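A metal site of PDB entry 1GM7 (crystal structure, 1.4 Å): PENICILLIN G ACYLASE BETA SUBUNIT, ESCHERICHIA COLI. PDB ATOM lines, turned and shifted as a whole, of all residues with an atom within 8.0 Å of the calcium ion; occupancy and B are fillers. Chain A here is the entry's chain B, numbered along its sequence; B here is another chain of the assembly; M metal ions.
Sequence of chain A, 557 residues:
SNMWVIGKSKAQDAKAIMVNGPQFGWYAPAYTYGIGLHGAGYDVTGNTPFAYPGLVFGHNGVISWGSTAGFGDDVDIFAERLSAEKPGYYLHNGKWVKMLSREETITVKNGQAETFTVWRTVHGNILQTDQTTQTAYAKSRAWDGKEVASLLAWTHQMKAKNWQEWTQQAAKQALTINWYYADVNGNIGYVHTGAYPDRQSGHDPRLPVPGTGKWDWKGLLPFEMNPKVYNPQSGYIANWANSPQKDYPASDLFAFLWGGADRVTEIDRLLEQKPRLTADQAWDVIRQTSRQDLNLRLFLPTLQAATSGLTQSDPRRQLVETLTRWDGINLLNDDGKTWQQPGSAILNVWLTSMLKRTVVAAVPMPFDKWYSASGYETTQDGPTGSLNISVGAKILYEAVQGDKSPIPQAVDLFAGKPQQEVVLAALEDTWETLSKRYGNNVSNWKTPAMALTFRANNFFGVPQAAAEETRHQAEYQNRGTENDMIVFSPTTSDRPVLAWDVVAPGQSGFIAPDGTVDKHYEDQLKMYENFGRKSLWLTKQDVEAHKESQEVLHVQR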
ATOM      1  N   GLY A  72       0.020   7.175 -22.526  1.00  0.00           N
ATOM      2  CA  GLY A  72       0.813   8.160 -21.801  1.00  0.00           C
ATOM      3  C   GLY A  72       1.333   9.219 -22.767  1.00  0.00           C
ATOM      4  O   GLY A  72       1.292   9.034 -23.980  1.00  0.00           O
ATOM      5  N   ASP A  73       1.789  10.317 -22.172  1.00  0.00           N
ATOM      6  CA  ASP A  73       2.334  11.384 -23.024  1.00  0.00           C
ATOM      7  C   ASP A  73       3.843  11.190 -23.180  1.00  0.00           C
ATOM      8  O   ASP A  73       4.667  11.581 -22.360  1.00  0.00           O
ATOM      9  CB  ASP A  73       2.002  12.720 -22.344  1.00  0.00           C
ATOM     10  CG  ASP A  73       2.467  13.842 -23.240  1.00  0.00           C
ATOM     11  OD1 ASP A  73       3.212  13.615 -24.246  1.00  0.00           O
ATOM     12  OD2 ASP A  73       2.112  15.045 -23.029  1.00  0.00           O
ATOM     13  N   ASP A  74       4.158  10.500 -24.294  1.00  0.00           N
ATOM     14  CA  ASP A  74       5.544  10.196 -24.617  1.00  0.00           C
ATOM     15  C   ASP A  74       5.996  10.932 -25.871  1.00  0.00           C
ATOM     16  O   ASP A  74       7.026  10.583 -26.480  1.00  0.00           O
ATOM     17  CB  ASP A  74       5.760   8.701 -24.785  1.00  0.00           C
ATOM     18  CG  ASP A  74       4.934   8.042 -25.855  1.00  0.00           C
ATOM     19  OD1 ASP A  74       4.049   8.695 -26.449  1.00  0.00           O
ATOM     20  OD2 ASP A  74       5.120   6.811 -26.143  1.00  0.00           O
ATOM     21  N   VAL A  75       5.265  11.974 -26.294  1.00  0.00           N
ATOM     22  CA  VAL A  75       5.554  12.750 -27.489  1.00  0.00           C
ATOM     23  C   VAL A  75       5.422  14.229 -27.275  1.00  0.00           C
ATOM     24  O   VAL A  75       4.308  14.635 -26.830  1.00  0.00           O
ATOM     25  CB  VAL A  75       4.655  12.327 -28.693  1.00  0.00           C
ATOM     26  CG1 VAL A  75       4.985  13.181 -29.907  1.00  0.00           C
ATOM     27  CG2 VAL A  75       4.798  10.859 -29.012  1.00  0.00           C
ATOM     28  N   ASP A  76       6.402  15.051 -27.508  1.00  0.00           N
ATOM     29  CA  ASP A  76       6.354  16.486 -27.392  1.00  0.00           C
ATOM     30  C   ASP A  76       6.786  17.104 -28.718  1.00  0.00           C
ATOM     31  O   ASP A  76       7.588  16.449 -29.436  1.00  0.00           O
ATOM     32  CB  ASP A  76       7.167  17.075 -26.245  1.00  0.00           C
ATOM     33  CG  ASP A  76       6.829  16.631 -24.858  1.00  0.00           C
ATOM     34  OD1 ASP A  76       5.653  16.191 -24.606  1.00  0.00           O
ATOM     35  OD2 ASP A  76       7.658  16.700 -23.942  1.00  0.00           O
ATOM     36  N   ILE A  77       6.324  18.308 -28.998  1.00  0.00           N
ATOM     37  CA  ILE A  77       6.659  19.021 -30.213  1.00  0.00           C
ATOM     38  C   ILE A  77       7.594  20.171 -29.872  1.00  0.00           C
ATOM     39  O   ILE A  77       7.354  20.948 -28.946  1.00  0.00           O
ATOM     40  CB  ILE A  77       5.396  19.588 -30.868  1.00  0.00           C
ATOM     41  CG1 ILE A  77       4.430  18.470 -31.287  1.00  0.00           C
ATOM     42  CG2 ILE A  77       5.754  20.439 -32.081  1.00  0.00           C
ATOM     43  CD1 ILE A  77       4.944  17.445 -32.200  1.00  0.00           C
ATOM     44  N   SER A 140       9.119  14.968 -31.228  1.00  0.00           N
ATOM     45  CA  SER A 140      10.054  14.220 -30.387  1.00  0.00           C
ATOM     46  C   SER A 140       9.407  13.090 -29.594  1.00  0.00           C
ATOM     47  O   SER A 140       8.593  13.292 -28.690  1.00  0.00           O
ATOM     48  CB  SER A 140      10.663  15.223 -29.391  1.00  0.00           C
ATOM     49  OG  SER A 140      11.754  14.617 -28.714  1.00  0.00           O
ATOM     50  N   PRO A 197       9.788  11.106 -21.082  1.00  0.00           N
ATOM     51  CA  PRO A 197      10.853  12.090 -20.930  1.00  0.00           C
ATOM     52  C   PRO A 197      10.965  12.700 -19.549  1.00  0.00           C
ATOM     53  O   PRO A 197       9.939  12.908 -18.898  1.00  0.00           O
ATOM     54  CB  PRO A 197      10.510  13.144 -21.992  1.00  0.00           C
ATOM     55  CG  PRO A 197       9.001  13.119 -22.058  1.00  0.00           C
ATOM     56  CD  PRO A 197       8.631  11.637 -21.812  1.00  0.00           C
ATOM     57  N   ARG A 199      11.381  15.977 -18.201  1.00  0.00           N
ATOM     58  CA  ARG A 199      11.212  17.325 -18.718  1.00  0.00           C
ATOM     59  C   ARG A 199      11.757  18.414 -17.795  1.00  0.00           C
ATOM     60  O   ARG A 199      11.783  18.260 -16.564  1.00  0.00           O
ATOM     61  CB  ARG A 199       9.687  17.554 -18.930  1.00  0.00           C
ATOM     62  CG  ARG A 199       9.085  16.620 -19.996  1.00  0.00           C
ATOM     63  CD  ARG A 199       7.628  16.914 -20.213  1.00  0.00           C
ATOM     64  NE  ARG A 199       7.003  16.183 -21.284  1.00  0.00           N
ATOM     65  CZ  ARG A 199       6.288  15.044 -21.117  1.00  0.00           C
ATOM     66  NH1 ARG A 199       6.148  14.480 -19.937  1.00  0.00           N
ATOM     67  NH2 ARG A 199       5.740  14.508 -22.205  1.00  0.00           N
ATOM     68  N   HIS A 203       7.925  22.885 -17.933  1.00  0.00           N
ATOM     69  CA  HIS A 203       7.457  22.406 -19.217  1.00  0.00           C
ATOM     70  C   HIS A 203       6.039  21.783 -19.108  1.00  0.00           C
ATOM     71  O   HIS A 203       5.856  20.726 -18.486  1.00  0.00           O
ATOM     72  CB  HIS A 203       8.476  21.375 -19.698  1.00  0.00           C
ATOM     73  CG  HIS A 203       8.207  20.684 -20.992  1.00  0.00           C
ATOM     74  ND1 HIS A 203       9.171  19.938 -21.649  1.00  0.00           N
ATOM     75  CD2 HIS A 203       7.097  20.601 -21.740  1.00  0.00           C
ATOM     76  CE1 HIS A 203       8.646  19.431 -22.744  1.00  0.00           C
ATOM     77  NE2 HIS A 203       7.354  19.814 -22.821  1.00  0.00           N
ATOM     78  N   ASP A 204       5.052  22.492 -19.697  1.00  0.00           N
ATOM     79  CA  ASP A 204       3.653  21.989 -19.707  1.00  0.00           C
ATOM     80  C   ASP A 204       3.626  21.031 -20.890  1.00  0.00           C
ATOM     81  O   ASP A 204       3.762  21.434 -22.022  1.00  0.00           O
ATOM     82  CB  ASP A 204       2.742  23.181 -19.922  1.00  0.00           C
ATOM     83  CG  ASP A 204       1.263  22.863 -19.968  1.00  0.00           C
ATOM     84  OD1 ASP A 204       0.911  21.736 -20.320  1.00  0.00           O
ATOM     85  OD2 ASP A 204       0.476  23.791 -19.644  1.00  0.00           O
ATOM     86  N   PRO A 205       3.417  19.729 -20.660  1.00  0.00           N
ATOM     87  CA  PRO A 205       3.524  18.710 -21.684  1.00  0.00           C
ATOM     88  C   PRO A 205       2.390  18.731 -22.650  1.00  0.00           C
ATOM     89  O   PRO A 205       2.454  17.945 -23.617  1.00  0.00           O
ATOM     90  CB  PRO A 205       3.623  17.393 -20.878  1.00  0.00           C
ATOM     91  CG  PRO A 205       2.773  17.715 -19.683  1.00  0.00           C
ATOM     92  CD  PRO A 205       3.158  19.160 -19.314  1.00  0.00           C
ATOM     93  N   ARG A 206       1.383  19.555 -22.539  1.00  0.00           N
ATOM     94  CA  ARG A 206       0.296  19.643 -23.489  1.00  0.00           C
ATOM     95  C   ARG A 206       0.565  20.560 -24.655  1.00  0.00           C
ATOM     96  O   ARG A 206      -0.256  20.620 -25.570  1.00  0.00           O
ATOM     97  CB  ARG A 206      -0.983  20.157 -22.759  1.00  0.00           C
ATOM     98  CG  ARG A 206      -1.392  19.239 -21.611  1.00  0.00           C
ATOM     99  CD  ARG A 206      -2.438  19.917 -20.745  1.00  0.00           C
ATOM    100  NE  ARG A 206      -1.925  21.131 -20.125  1.00  0.00           N
ATOM    101  CZ  ARG A 206      -2.636  21.909 -19.347  1.00  0.00           C
ATOM    102  NH1 ARG A 206      -3.917  21.626 -19.041  1.00  0.00           N
ATOM    103  NH2 ARG A 206      -2.101  22.992 -18.799  1.00  0.00           N
ATOM    104  N   LEU A 207       1.668  21.341 -24.581  1.00  0.00           N
ATOM    105  CA  LEU A 207       1.912  22.398 -25.563  1.00  0.00           C
ATOM    106  C   LEU A 207       3.365  22.412 -26.022  1.00  0.00           C
ATOM    107  O   LEU A 207       4.227  21.929 -25.287  1.00  0.00           O
ATOM    108  CB  LEU A 207       1.562  23.715 -24.812  1.00  0.00           C
ATOM    109  CG  LEU A 207       0.100  23.873 -24.387  1.00  0.00           C
ATOM    110  CD1 LEU A 207      -0.032  24.882 -23.258  1.00  0.00           C
ATOM    111  CD2 LEU A 207      -0.773  24.220 -25.577  1.00  0.00           C
ATOM    112  N   PRO A 208       3.615  22.909 -27.214  1.00  0.00           N
ATOM    113  CA  PRO A 208       4.989  22.868 -27.768  1.00  0.00           C
ATOM    114  C   PRO A 208       5.999  23.548 -26.898  1.00  0.00           C
ATOM    115  O   PRO A 208       5.716  24.469 -26.127  1.00  0.00           O
ATOM    116  CB  PRO A 208       4.892  23.500 -29.159  1.00  0.00           C
ATOM    117  CG  PRO A 208       3.409  23.335 -29.466  1.00  0.00           C
ATOM    118  CD  PRO A 208       2.697  23.567 -28.133  1.00  0.00           C
ATOM    119  N   VAL A 209       7.277  23.178 -27.055  1.00  0.00           N
ATOM    120  CA  VAL A 209       8.402  23.782 -26.366  1.00  0.00           C
ATOM    121  C   VAL A 209       9.390  24.391 -27.351  1.00  0.00           C
ATOM    122  O   VAL A 209       9.599  23.838 -28.453  1.00  0.00           O
ATOM    123  CB  VAL A 209       9.206  22.761 -25.516  1.00  0.00           C
ATOM    124  CG1 VAL A 209       8.646  22.742 -24.096  1.00  0.00           C
ATOM    125  CG2 VAL A 209       9.144  21.327 -26.039  1.00  0.00           C
ATOM    126  N   TRP A 217      14.675  17.957 -23.394  1.00  0.00           N
ATOM    127  CA  TRP A 217      14.519  16.984 -22.338  1.00  0.00           C
ATOM    128  C   TRP A 217      15.843  16.723 -21.622  1.00  0.00           C
ATOM    129  O   TRP A 217      16.905  16.743 -22.277  1.00  0.00           O
ATOM    130  CB  TRP A 217      14.002  15.700 -22.930  1.00  0.00           C
ATOM    131  CG  TRP A 217      12.615  15.712 -23.494  1.00  0.00           C
ATOM    132  CD1 TRP A 217      11.578  16.577 -23.255  1.00  0.00           C
ATOM    133  CD2 TRP A 217      12.108  14.772 -24.443  1.00  0.00           C
ATOM    134  NE1 TRP A 217      10.454  16.183 -23.942  1.00  0.00           N
ATOM    135  CE2 TRP A 217      10.753  15.080 -24.685  1.00  0.00           C
ATOM    136  CE3 TRP A 217      12.672  13.651 -25.065  1.00  0.00           C
ATOM    137  CZ2 TRP A 217       9.936  14.328 -25.536  1.00  0.00           C
ATOM    138  CZ3 TRP A 217      11.863  12.918 -25.909  1.00  0.00           C
ATOM    139  CH2 TRP A 217      10.514  13.236 -26.115  1.00  0.00           C
ATOM    140  N   ALA A 250      -2.360  11.806 -18.807  1.00  0.00           N
ATOM    141  CA  ALA A 250      -2.707  11.240 -20.075  1.00  0.00           C
ATOM    142  C   ALA A 250      -1.947  11.845 -21.257  1.00  0.00           C
ATOM    143  O   ALA A 250      -1.392  12.932 -21.168  1.00  0.00           O
ATOM    144  CB  ALA A 250      -4.203  11.557 -20.335  1.00  0.00           C
ATOM    145  N   SER A 251      -2.060  11.132 -22.370  1.00  0.00           N
ATOM    146  CA  SER A 251      -1.711  11.675 -23.692  1.00  0.00           C
ATOM    147  C   SER A 251      -2.204  13.130 -23.801  1.00  0.00           C
ATOM    148  O   SER A 251      -3.288  13.483 -23.292  1.00  0.00           O
ATOM    149  CB  SER A 251      -2.526  10.874 -24.699  1.00  0.00           C
ATOM    150  OG  SER A 251      -2.352  11.358 -26.013  1.00  0.00           O
ATOM    151  N   ASP A 252      -1.450  13.942 -24.564  1.00  0.00           N
ATOM    152  CA  ASP A 252      -1.846  15.331 -24.755  1.00  0.00           C
ATOM    153  C   ASP A 252      -2.923  15.540 -25.804  1.00  0.00           C
ATOM    154  O   ASP A 252      -3.406  16.674 -25.985  1.00  0.00           O
ATOM    155  CB  ASP A 252      -0.620  16.209 -25.052  1.00  0.00           C
ATOM    156  CG  ASP A 252      -0.020  15.894 -26.381  1.00  0.00           C
ATOM    157  OD1 ASP A 252      -0.716  15.778 -27.357  1.00  0.00           O
ATOM    158  OD2 ASP A 252       1.250  15.785 -26.429  1.00  0.00           O
ATOM    159  N   LEU A 253      -3.437  14.516 -26.436  1.00  0.00           N
ATOM    160  CA  LEU A 253      -4.506  14.644 -27.428  1.00  0.00           C
ATOM    161  C   LEU A 253      -5.689  15.383 -26.813  1.00  0.00           C
ATOM    162  O   LEU A 253      -6.242  14.976 -25.757  1.00  0.00           O
ATOM    163  CB  LEU A 253      -4.999  13.266 -27.857  1.00  0.00           C
ATOM    164  CG  LEU A 253      -4.057  12.424 -28.707  1.00  0.00           C
ATOM    165  CD1 LEU A 253      -4.705  11.054 -28.907  1.00  0.00           C
ATOM    166  CD2 LEU A 253      -3.779  13.061 -30.051  1.00  0.00           C
ATOM    167  N   SER B 149       1.069   9.595 -30.525  1.00  0.00           N
ATOM    168  CA  SER B 149      -0.066  10.488 -30.495  1.00  0.00           C
ATOM    169  C   SER B 149       0.215  11.786 -29.775  1.00  0.00           C
ATOM    170  O   SER B 149       0.524  11.824 -28.606  1.00  0.00           O
ATOM    171  CB  SER B 149      -1.211   9.780 -29.713  1.00  0.00           C
ATOM    172  OG  SER B 149      -1.853   8.796 -30.497  1.00  0.00           O
ATOM    173  N   THR B 150       0.051  12.886 -30.535  1.00  0.00           N
ATOM    174  CA  THR B 150       0.169  14.225 -29.976  1.00  0.00           C
ATOM    175  C   THR B 150      -0.750  15.143 -30.766  1.00  0.00           C
ATOM    176  O   THR B 150      -0.989  14.969 -31.956  1.00  0.00           O
ATOM    177  CB  THR B 150       1.627  14.745 -29.978  1.00  0.00           C
ATOM    178  OG1 THR B 150       1.677  15.987 -29.252  1.00  0.00           O
ATOM    179  CG2 THR B 150       2.164  14.986 -31.389  1.00  0.00           C
ATOM    180  N   SER B 151      -1.235  16.188 -30.085  1.00  0.00           N
ATOM    181  CA  SER B 151      -2.008  17.236 -30.729  1.00  0.00           C
ATOM    182  C   SER B 151      -1.504  18.602 -30.215  1.00  0.00           C
ATOM    183  O   SER B 151      -2.278  19.563 -30.286  1.00  0.00           O
ATOM    184  CB  SER B 151      -3.513  17.138 -30.597  1.00  0.00           C
ATOM    185  OG  SER B 151      -3.919  17.290 -29.228  1.00  0.00           O
ATOM    186  N   GLU B 152      -0.217  18.717 -29.851  1.00  0.00           N
ATOM    187  CA  GLU B 152       0.219  19.956 -29.255  1.00  0.00           C
ATOM    188  C   GLU B 152       0.061  21.208 -30.105  1.00  0.00           C
ATOM    189  O   GLU B 152      -0.208  22.281 -29.517  1.00  0.00           O
ATOM    190  CB  GLU B 152       1.704  19.879 -28.787  1.00  0.00           C
ATOM    191  CG  GLU B 152       1.908  18.912 -27.643  1.00  0.00           C
ATOM    192  CD  GLU B 152       3.330  18.839 -27.227  1.00  0.00           C
ATOM    193  OE1 GLU B 152       4.213  19.600 -27.690  1.00  0.00           O
ATOM    194  OE2 GLU B 152       3.707  18.015 -26.360  1.00  0.00           O
ATOM    195  N   ASN B 155      -3.482  22.058 -29.777  1.00  0.00           N
ATOM    196  CA  ASN B 155      -3.728  22.490 -28.401  1.00  0.00           C
ATOM    197  C   ASN B 155      -3.349  23.958 -28.258  1.00  0.00           C
ATOM    198  O   ASN B 155      -4.036  24.726 -27.557  1.00  0.00           O
ATOM    199  CB  ASN B 155      -2.975  21.631 -27.396  1.00  0.00           C
ATOM    200  CG  ASN B 155      -3.400  20.165 -27.413  1.00  0.00           C
ATOM    201  OD1 ASN B 155      -4.369  19.792 -28.053  1.00  0.00           O
ATOM    202  ND2 ASN B 155      -2.633  19.398 -26.676  1.00  0.00           N
HETATM  203 CA    CA M   1       3.263  16.056 -25.088  1.00  0.00          CA
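The calcium ion is bound by OE2 of Glu 152 of chain B, OD2 of Asp 252, OD1 of Asp 76, O of Val 75, O of Pro 205, OD2 of Asp 73 and OD1 of Asp 73.
Within 4 Å of the calcium ion: Asp 73, Val 75, Asp 76, Pro 205, Asp 252 and Glu 152 of chain B.
The nearest printed residue that does not touch the calcium ion is Arg 199 (4.1 Å).
The side-chain hydroxyl (OG1) of Thr 150 of chain B sits close to the backbone NH (N) of Glu 152 of chain B (3.4 Å).
OE1 of Glu 152 of chain B is in hydrogen-bond range of N of Ile 77 (2.8 Å).
The side-chain carboxylate (OD1) of Asp 252 sits at hydrogen-bond distance from the side-chain hydroxyl (OG1) of Thr 150 of chain B (3.1 Å).
The side-chain carboxylate of Asp 252 lies within hydrogen-bond range of the backbone NH of Ser 151 of chain B (2.8 Å).
The backbone carbonyl oxygen (O) of Asp 252 is in hydrogen-bond range of the side-chain amide nitrogen (ND2) of Asn 155 of chain B (2.9 Å).
NE2 of His 203 lies close to OD2 of Asp 76 (3.3 Å).
The side-chain carboxylate (OD2) of Asp 76 lies within hydrogen-bond range of the indole nitrogen (NE1) of Trp 217.
The backbone carbonyl oxygen (O) of Asp 76 is in hydrogen-bond range of the backbone NH (N) of Ser 140, 2.8 Å away.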
